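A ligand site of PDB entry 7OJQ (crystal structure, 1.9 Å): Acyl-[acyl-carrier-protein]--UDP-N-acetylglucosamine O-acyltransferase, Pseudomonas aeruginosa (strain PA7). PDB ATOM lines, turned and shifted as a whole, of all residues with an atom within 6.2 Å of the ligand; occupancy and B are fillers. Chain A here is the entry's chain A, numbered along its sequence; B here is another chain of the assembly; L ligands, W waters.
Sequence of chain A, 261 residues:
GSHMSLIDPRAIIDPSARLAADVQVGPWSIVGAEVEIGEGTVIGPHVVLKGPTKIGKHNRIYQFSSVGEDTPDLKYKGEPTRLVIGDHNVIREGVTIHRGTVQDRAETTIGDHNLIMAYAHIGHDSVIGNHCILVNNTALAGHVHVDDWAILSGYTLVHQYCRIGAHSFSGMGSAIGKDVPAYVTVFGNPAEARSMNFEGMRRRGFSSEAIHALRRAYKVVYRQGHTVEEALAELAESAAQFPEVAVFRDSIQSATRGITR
The side-chain amide oxygen of Gln 160 of chain B sits close to a nitrogen (N2) of the ligand, at 3.4 Å.
O1 of the ligand sits close to OG of Ser 153.
The backbone NH of Gly 154 is in hydrogen-bond range of an oxygen (O1) of the ligand (3.0 Å).
O of Ile 151 is in hydrogen-bond range of N of Ser 170 (3.1 Å).
The backbone carbonyl oxygen of His 121 of chain B lies within hydrogen-bond range of the backbone NH of Leu 140 of chain B (2.9 Å).
OG of Ser 153 is in hydrogen-bond range of O of Ser 170, 2.7 Å away.
O of Val 158 of chain B is in hydrogen-bond range of N of Ala 141 of chain B, at 3.0 Å.
O of Ala 139 of chain B is in hydrogen-bond range of N of Val 158 of chain B, 2.8 Å away.
The backbone carbonyl oxygen (O) of Asn 136 sits at hydrogen-bond distance from the backbone NH (N) of Tyr 155, 2.9 Å away.
N of Val 135 sits at hydrogen-bond distance from O of Leu 152 (2.9 Å).
ND2 of Asn 136 lies within hydrogen-bond range of ND1 of His 121 of chain B (3.4 Å).
CD2 of Leu 115 touches N1 of the ligand, 3.6 Å away.
Val 135 touches the ligand.
Asn 136 touches the ligand.
CG2 of Ile 151 touches C6 of the ligand (3.97 Å).
CD1 of Tyr 155 touches CL1 of the ligand (3.98 Å).
CB of Met 172 touches S1 of the ligand (3.8 Å).
NE2 of His 121 of chain B touches C3 of the ligand, at 3.7 Å.
CB of Ala 139 of chain B touches CL1 of the ligand, 3.9 Å away.
Ala 141 of chain B touches the ligand.
Hydrophobic or aromatic side chains within 4 Å of the ligand: Leu 115, Val 135, Ile 151, Tyr 155, Met 172, His 121 of chain B, Ala 139 of chain B and Ala 141 of chain B.
12 residues have an atom within 4 Å of the ligand: Leu 115, Val 135, Asn 136, Ile 151, Ser 153, Gly 154, Tyr 155, Met 172, His 121 of chain B, Ala 139 of chain B, Ala 141 of chain B and Gln 160 of chain B.
The nearest printed residue that does not touch the ligand is Met 117 (4.03 Å).
Water W3 lies within hydrogen-bond range of the side-chain sulfur (SD) of Met 172 (3.1 Å) and a sulfur (S1) of the ligand (3.7 Å).
Water W4 bridges N of Gln 160 of chain B (3.0 Å) and NE2 of His 159 of chain B (3.5 Å).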
ATOM      1  N   LEU A 115     -11.554   9.331  22.297  1.00  0.00           N
ATOM      2  CA  LEU A 115     -12.459   8.986  21.223  1.00  0.00           C
ATOM      3  C   LEU A 115     -12.304   7.490  20.982  1.00  0.00           C
ATOM      4  O   LEU A 115     -11.256   7.006  20.551  1.00  0.00           O
ATOM      5  CB  LEU A 115     -12.146   9.816  19.947  1.00  0.00           C
ATOM      6  CG  LEU A 115     -12.943   9.437  18.673  1.00  0.00           C
ATOM      7  CD1 LEU A 115     -14.487   9.415  18.924  1.00  0.00           C
ATOM      8  CD2 LEU A 115     -12.530  10.328  17.476  1.00  0.00           C
ATOM      9  N   MET A 117     -13.947   4.659  18.952  1.00  0.00           N
ATOM     10  CA  MET A 117     -14.753   4.544  17.764  1.00  0.00           C
ATOM     11  C   MET A 117     -15.426   3.205  17.647  1.00  0.00           C
ATOM     12  O   MET A 117     -15.158   2.298  18.416  1.00  0.00           O
ATOM     13  CB  MET A 117     -13.930   4.930  16.519  1.00  0.00           C
ATOM     14  CG  MET A 117     -13.452   6.366  16.639  1.00  0.00           C
ATOM     15  SD  MET A 117     -12.314   6.865  15.325  1.00  0.00           S
ATOM     16  CE  MET A 117     -13.501   7.342  14.068  1.00  0.00           C
ATOM     17  N   ILE A 133      -7.133   8.104  20.710  1.00  0.00           N
ATOM     18  CA  ILE A 133      -8.112   7.738  19.702  1.00  0.00           C
ATOM     19  C   ILE A 133      -7.932   6.254  19.458  1.00  0.00           C
ATOM     20  O   ILE A 133      -6.832   5.809  19.139  1.00  0.00           O
ATOM     21  CB  ILE A 133      -8.004   8.568  18.368  1.00  0.00           C
ATOM     22  CG1 ILE A 133      -8.087  10.089  18.642  1.00  0.00           C
ATOM     23  CG2 ILE A 133      -9.123   8.114  17.359  1.00  0.00           C
ATOM     24  CD1 ILE A 133      -7.678  11.024  17.505  1.00  0.00           C
ATOM     25  N   VAL A 135      -9.489   3.790  17.004  1.00  0.00           N
ATOM     26  CA  VAL A 135     -10.248   3.773  15.753  1.00  0.00           C
ATOM     27  C   VAL A 135     -11.043   2.444  15.690  1.00  0.00           C
ATOM     28  O   VAL A 135     -10.727   1.515  16.450  1.00  0.00           O
ATOM     29  CB  VAL A 135      -9.344   4.086  14.506  1.00  0.00           C
ATOM     30  CG1 VAL A 135     -10.143   4.158  13.202  1.00  0.00           C
ATOM     31  CG2 VAL A 135      -8.594   5.421  14.715  1.00  0.00           C
ATOM     32  N   ASN A 136     -12.096   2.416  14.896  1.00  0.00           N
ATOM     33  CA  ASN A 136     -13.043   1.287  14.696  1.00  0.00           C
ATOM     34  C   ASN A 136     -12.399  -0.062  14.867  1.00  0.00           C
ATOM     35  O   ASN A 136     -11.370  -0.331  14.220  1.00  0.00           O
ATOM     36  CB  ASN A 136     -13.685   1.330  13.294  1.00  0.00           C
ATOM     37  CG  ASN A 136     -14.511   2.555  12.980  1.00  0.00           C
ATOM     38  OD1 ASN A 136     -14.066   3.677  13.107  1.00  0.00           O
ATOM     39  ND2 ASN A 136     -15.711   2.335  12.479  1.00  0.00           N
ATOM     40  N   ILE A 151      -2.646   6.985  19.101  1.00  0.00           N
ATOM     41  CA  ILE A 151      -3.647   6.773  18.060  1.00  0.00           C
ATOM     42  C   ILE A 151      -3.469   5.346  17.591  1.00  0.00           C
ATOM     43  O   ILE A 151      -2.407   4.999  17.097  1.00  0.00           O
ATOM     44  CB  ILE A 151      -3.550   7.770  16.870  1.00  0.00           C
ATOM     45  CG1 ILE A 151      -3.784   9.214  17.329  1.00  0.00           C
ATOM     46  CG2 ILE A 151      -4.526   7.356  15.723  1.00  0.00           C
ATOM     47  CD1 ILE A 151      -3.365  10.269  16.275  1.00  0.00           C
ATOM     48  N   LEU A 152      -4.497   4.536  17.772  1.00  0.00           N
ATOM     49  CA  LEU A 152      -4.511   3.162  17.295  1.00  0.00           C
ATOM     50  C   LEU A 152      -5.486   3.112  16.132  1.00  0.00           C
ATOM     51  O   LEU A 152      -6.702   3.299  16.327  1.00  0.00           O
ATOM     52  CB  LEU A 152      -4.869   2.150  18.419  1.00  0.00           C
ATOM     53  CG  LEU A 152      -3.960   2.117  19.674  1.00  0.00           C
ATOM     54  CD1 LEU A 152      -4.513   1.176  20.718  1.00  0.00           C
ATOM     55  CD2 LEU A 152      -2.537   1.680  19.337  1.00  0.00           C
ATOM     56  N   SER A 153      -4.943   2.924  14.905  1.00  0.00           N
ATOM     57  CA  SER A 153      -5.721   2.898  13.649  1.00  0.00           C
ATOM     58  C   SER A 153      -6.650   1.718  13.637  1.00  0.00           C
ATOM     59  O   SER A 153      -6.476   0.801  14.438  1.00  0.00           O
ATOM     60  CB  SER A 153      -4.807   2.874  12.422  1.00  0.00           C
ATOM     61  OG  SER A 153      -4.102   4.109  12.302  1.00  0.00           O
ATOM     62  N   GLY A 154      -7.648   1.768  12.767  1.00  0.00           N
ATOM     63  CA  GLY A 154      -8.690   0.752  12.660  1.00  0.00           C
ATOM     64  C   GLY A 154      -8.157  -0.655  12.682  1.00  0.00           C
ATOM     65  O   GLY A 154      -7.138  -0.950  12.045  1.00  0.00           O
ATOM     66  N   TYR A 155      -8.823  -1.502  13.494  1.00  0.00           N
ATOM     67  CA  TYR A 155      -8.527  -2.930  13.605  1.00  0.00           C
ATOM     68  C   TYR A 155      -7.162  -3.260  14.185  1.00  0.00           C
ATOM     69  O   TYR A 155      -6.603  -4.313  13.876  1.00  0.00           O
ATOM     70  CB  TYR A 155      -8.752  -3.651  12.246  1.00  0.00           C
ATOM     71  CG  TYR A 155     -10.217  -3.759  11.855  1.00  0.00           C
ATOM     72  CD1 TYR A 155     -10.911  -2.667  11.354  1.00  0.00           C
ATOM     73  CD2 TYR A 155     -10.891  -4.980  11.950  1.00  0.00           C
ATOM     74  CE1 TYR A 155     -12.271  -2.755  11.058  1.00  0.00           C
ATOM     75  CE2 TYR A 155     -12.242  -5.086  11.655  1.00  0.00           C
ATOM     76  CZ  TYR A 155     -12.926  -3.977  11.180  1.00  0.00           C
ATOM     77  OH  TYR A 155     -14.249  -4.083  10.853  1.00  0.00           O
ATOM     78  N   PHE A 169       1.690   5.618  17.498  1.00  0.00           N
ATOM     79  CA  PHE A 169       0.730   5.424  16.416  1.00  0.00           C
ATOM     80  C   PHE A 169       0.849   3.999  15.867  1.00  0.00           C
ATOM     81  O   PHE A 169       1.946   3.544  15.607  1.00  0.00           O
ATOM     82  CB  PHE A 169       1.041   6.445  15.261  1.00  0.00           C
ATOM     83  CG  PHE A 169       0.206   6.271  14.009  1.00  0.00           C
ATOM     84  CD1 PHE A 169      -1.058   6.843  13.905  1.00  0.00           C
ATOM     85  CD2 PHE A 169       0.673   5.500  12.944  1.00  0.00           C
ATOM     86  CE1 PHE A 169      -1.833   6.666  12.733  1.00  0.00           C
ATOM     87  CE2 PHE A 169      -0.125   5.280  11.806  1.00  0.00           C
ATOM     88  CZ  PHE A 169      -1.361   5.877  11.705  1.00  0.00           C
ATOM     89  N   SER A 170      -0.280   3.326  15.661  1.00  0.00           N
ATOM     90  CA  SER A 170      -0.271   2.023  15.006  1.00  0.00           C
ATOM     91  C   SER A 170      -1.012   2.199  13.687  1.00  0.00           C
ATOM     92  O   SER A 170      -2.019   2.929  13.638  1.00  0.00           O
ATOM     93  CB  SER A 170      -0.945   0.951  15.858  1.00  0.00           C
ATOM     94  OG  SER A 170      -2.328   1.212  16.006  1.00  0.00           O
ATOM     95  N   MET A 172      -3.175   0.676  10.280  1.00  0.00           N
ATOM     96  CA  MET A 172      -4.398  -0.145  10.266  1.00  0.00           C
ATOM     97  C   MET A 172      -4.077  -1.644  10.196  1.00  0.00           C
ATOM     98  O   MET A 172      -3.113  -2.044   9.551  1.00  0.00           O
ATOM     99  CB  MET A 172      -5.411   0.333   9.184  1.00  0.00           C
ATOM    100  CG  MET A 172      -5.022   0.032   7.774  1.00  0.00           C
ATOM    101  SD  MET A 172      -6.278   0.511   6.530  1.00  0.00           S
ATOM    102  CE  MET A 172      -5.534  -0.231   5.116  1.00  0.00           C
ATOM    103  N   PRO B  72     -17.446  11.391  12.930  1.00  0.00           N
ATOM    104  CA  PRO B  72     -16.826  11.578  14.259  1.00  0.00           C
ATOM    105  C   PRO B  72     -15.497  12.323  14.161  1.00  0.00           C
ATOM    106  O   PRO B  72     -14.963  12.800  15.161  1.00  0.00           O
ATOM    107  CB  PRO B  72     -16.619  10.135  14.772  1.00  0.00           C
ATOM    108  CG  PRO B  72     -17.278   9.233  13.755  1.00  0.00           C
ATOM    109  CD  PRO B  72     -17.267   9.998  12.472  1.00  0.00           C
ATOM    110  N   HIS B 121     -18.246  -1.106   7.435  1.00  0.00           N
ATOM    111  CA  HIS B 121     -18.182   0.307   7.732  1.00  0.00           C
ATOM    112  C   HIS B 121     -17.935   1.128   6.457  1.00  0.00           C
ATOM    113  O   HIS B 121     -16.970   0.870   5.730  1.00  0.00           O
ATOM    114  CB  HIS B 121     -17.072   0.581   8.743  1.00  0.00           C
ATOM    115  CG  HIS B 121     -16.820   2.034   8.933  1.00  0.00           C
ATOM    116  ND1 HIS B 121     -17.668   2.824   9.691  1.00  0.00           N
ATOM    117  CD2 HIS B 121     -15.847   2.817   8.425  1.00  0.00           C
ATOM    118  CE1 HIS B 121     -17.149   4.030   9.669  1.00  0.00           C
ATOM    119  NE2 HIS B 121     -16.066   4.081   8.904  1.00  0.00           N
ATOM    120  N   HIS B 124     -17.232   8.365   5.640  1.00  0.00           N
ATOM    121  CA  HIS B 124     -17.704   9.580   5.007  1.00  0.00           C
ATOM    122  C   HIS B 124     -17.103   9.811   3.618  1.00  0.00           C
ATOM    123  O   HIS B 124     -15.929   9.482   3.376  1.00  0.00           O
ATOM    124  CB  HIS B 124     -17.420  10.797   5.898  1.00  0.00           C
ATOM    125  CG  HIS B 124     -15.961  11.074   6.133  1.00  0.00           C
ATOM    126  ND1 HIS B 124     -15.262  10.423   7.139  1.00  0.00           N
ATOM    127  CD2 HIS B 124     -15.127  11.919   5.505  1.00  0.00           C
ATOM    128  CE1 HIS B 124     -14.034  10.912   7.094  1.00  0.00           C
ATOM    129  NE2 HIS B 124     -13.898  11.803   6.116  1.00  0.00           N
ATOM    130  N   ALA B 139     -13.993  -2.430   5.951  1.00  0.00           N
ATOM    131  CA  ALA B 139     -14.034  -1.060   6.426  1.00  0.00           C
ATOM    132  C   ALA B 139     -13.393  -0.099   5.414  1.00  0.00           C
ATOM    133  O   ALA B 139     -12.252  -0.306   4.994  1.00  0.00           O
ATOM    134  CB  ALA B 139     -13.382  -0.967   7.788  1.00  0.00           C
ATOM    135  N   LEU B 140     -14.191   0.868   4.941  1.00  0.00           N
ATOM    136  CA  LEU B 140     -13.771   1.928   4.028  1.00  0.00           C
ATOM    137  C   LEU B 140     -13.493   3.144   4.927  1.00  0.00           C
ATOM    138  O   LEU B 140     -14.436   3.683   5.515  1.00  0.00           O
ATOM    139  CB  LEU B 140     -14.836   2.248   2.950  1.00  0.00           C
ATOM    140  CG  LEU B 140     -15.460   1.062   2.153  1.00  0.00           C
ATOM    141  CD1 LEU B 140     -16.441   1.567   1.116  1.00  0.00           C
ATOM    142  CD2 LEU B 140     -14.396   0.232   1.464  1.00  0.00           C
ATOM    143  N   ALA B 141     -12.225   3.494   5.111  1.00  0.00           N
ATOM    144  CA  ALA B 141     -11.838   4.585   6.038  1.00  0.00           C
ATOM    145  C   ALA B 141     -12.505   5.941   5.726  1.00  0.00           C
ATOM    146  O   ALA B 141     -12.961   6.611   6.641  1.00  0.00           O
ATOM    147  CB  ALA B 141     -10.323   4.727   6.108  1.00  0.00           C
ATOM    148  N   GLY B 142     -12.653   6.277   4.451  1.00  0.00           N
ATOM    149  CA  GLY B 142     -13.284   7.523   4.031  1.00  0.00           C
ATOM    150  C   GLY B 142     -12.784   7.907   2.654  1.00  0.00           C
ATOM    151  O   GLY B 142     -11.683   7.527   2.279  1.00  0.00           O
ATOM    152  N   LEU B 157      -9.661  -3.959   4.804  1.00  0.00           N
ATOM    153  CA  LEU B 157      -9.518  -2.580   5.275  1.00  0.00           C
ATOM    154  C   LEU B 157      -9.035  -1.709   4.122  1.00  0.00           C
ATOM    155  O   LEU B 157      -8.098  -2.068   3.420  1.00  0.00           O
ATOM    156  CB  LEU B 157      -8.535  -2.492   6.455  1.00  0.00           C
ATOM    157  CG  LEU B 157      -8.735  -3.540   7.581  1.00  0.00           C
ATOM    158  CD1 LEU B 157      -7.652  -3.354   8.673  1.00  0.00           C
ATOM    159  CD2 LEU B 157     -10.137  -3.473   8.138  1.00  0.00           C
ATOM    160  N   VAL B 158      -9.697  -0.592   3.894  1.00  0.00           N
ATOM    161  CA  VAL B 158      -9.306   0.270   2.787  1.00  0.00           C
ATOM    162  C   VAL B 158      -8.915   1.658   3.311  1.00  0.00           C
ATOM    163  O   VAL B 158      -9.765   2.352   3.899  1.00  0.00           O
ATOM    164  CB  VAL B 158     -10.388   0.383   1.684  1.00  0.00           C
ATOM    165  CG1 VAL B 158      -9.843   1.182   0.503  1.00  0.00           C
ATOM    166  CG2 VAL B 158     -10.891  -1.001   1.206  1.00  0.00           C
ATOM    167  N   HIS B 159      -7.654   2.067   3.063  1.00  0.00           N
ATOM    168  CA  HIS B 159      -7.084   3.378   3.427  1.00  0.00           C
ATOM    169  C   HIS B 159      -7.906   4.469   2.745  1.00  0.00           C
ATOM    170  O   HIS B 159      -8.442   4.242   1.654  1.00  0.00           O
ATOM    171  CB  HIS B 159      -5.613   3.446   2.972  1.00  0.00           C
ATOM    172  CG  HIS B 159      -4.840   4.646   3.411  1.00  0.00           C
ATOM    173  ND1 HIS B 159      -4.977   5.884   2.773  1.00  0.00           N
ATOM    174  CD2 HIS B 159      -3.911   4.778   4.401  1.00  0.00           C
ATOM    175  CE1 HIS B 159      -4.162   6.713   3.410  1.00  0.00           C
ATOM    176  NE2 HIS B 159      -3.490   6.093   4.380  1.00  0.00           N
ATOM    177  N   GLN B 160      -8.042   5.624   3.390  1.00  0.00           N
ATOM    178  CA  GLN B 160      -8.730   6.805   2.845  1.00  0.00           C
ATOM    179  C   GLN B 160      -8.218   7.149   1.427  1.00  0.00           C
ATOM    180  O   GLN B 160      -7.038   6.965   1.143  1.00  0.00           O
ATOM    181  CB  GLN B 160      -8.487   8.027   3.747  1.00  0.00           C
ATOM    182  CG  GLN B 160      -9.329   8.098   5.027  1.00  0.00           C
ATOM    183  CD  GLN B 160      -9.459   9.536   5.483  1.00  0.00           C
ATOM    184  OE1 GLN B 160      -8.473  10.212   5.803  1.00  0.00           O
ATOM    185  NE2 GLN B 160     -10.679  10.034   5.503  1.00  0.00           N
HETATM  186  C1  LIG L   1     -10.140  10.574  14.031  1.00  0.00           C
HETATM  187  C2  LIG L   1     -11.753   4.676  10.064  1.00  0.00           C
HETATM  188  C3  LIG L   1     -12.614   3.585  10.102  1.00  0.00           C
HETATM  189  C4  LIG L   1      -7.900   9.834  13.620  1.00  0.00           C
HETATM  190  C5  LIG L   1      -9.725   8.553  12.740  1.00  0.00           C
HETATM  191  C6  LIG L   1      -7.008   8.940  13.066  1.00  0.00           C
HETATM  192  C7  LIG L   1      -8.825   7.663  12.192  1.00  0.00           C
HETATM  193  C8  LIG L   1     -10.415   4.489   9.779  1.00  0.00           C
HETATM  194  C9  LIG L   1     -12.121   2.315   9.832  1.00  0.00           C
HETATM  195  C10 LIG L   1      -9.251   9.633  13.460  1.00  0.00           C
HETATM  196  C11 LIG L   1      -7.463   7.858  12.358  1.00  0.00           C
HETATM  197  C12 LIG L   1      -9.911   3.224   9.543  1.00  0.00           C
HETATM  198  C13 LIG L   1     -10.790   2.157   9.538  1.00  0.00           C
HETATM  199  C14 LIG L   1      -9.681   8.648   8.800  1.00  0.00           C
HETATM  200  C15 LIG L   1      -7.701   8.090   9.133  1.00  0.00           C
HETATM  201  C16 LIG L   1      -7.236   5.081  10.385  1.00  0.00           C
HETATM  202  C17 LIG L   1     -11.103   8.475   8.496  1.00  0.00           C
HETATM  203  C18 LIG L   1      -6.445   6.933  11.759  1.00  0.00           C
HETATM  204  C19 LIG L   1      -6.553   7.188   9.282  1.00  0.00           C
HETATM  205  C20 LIG L   1      -7.528   4.549   9.011  1.00  0.00           C
HETATM  206  N1  LIG L   1     -10.850  11.374  14.497  1.00  0.00           N
HETATM  207  N2  LIG L   1      -9.029   9.753   9.123  1.00  0.00           N
HETATM  208  N3  LIG L   1      -7.730   9.378   9.350  1.00  0.00           N
HETATM  209  N4  LIG L   1      -6.857   6.414  10.466  1.00  0.00           N
HETATM  210  O1  LIG L   1      -7.339   4.350  11.347  1.00  0.00           O
HETATM  211  O2  LIG L   1      -8.899   7.523   8.782  1.00  0.00           O
HETATM  212  S1  LIG L   1      -8.218   2.869   9.159  1.00  0.00           S
HETATM  213 CL1  LIG L   1     -10.144   0.590   9.199  1.00  0.00          CL
HETATM  214  O   HOH W   1      -5.536   8.652   6.333  1.00  0.00           O
HETATM  215  O   HOH W   2      -4.005   4.740   9.617  1.00  0.00           O
HETATM  216  O   HOH W   3      -5.378   3.447   6.863  1.00  0.00           O
HETATM  217  O   HOH W   4      -6.533   5.781   6.025  1.00  0.00           O
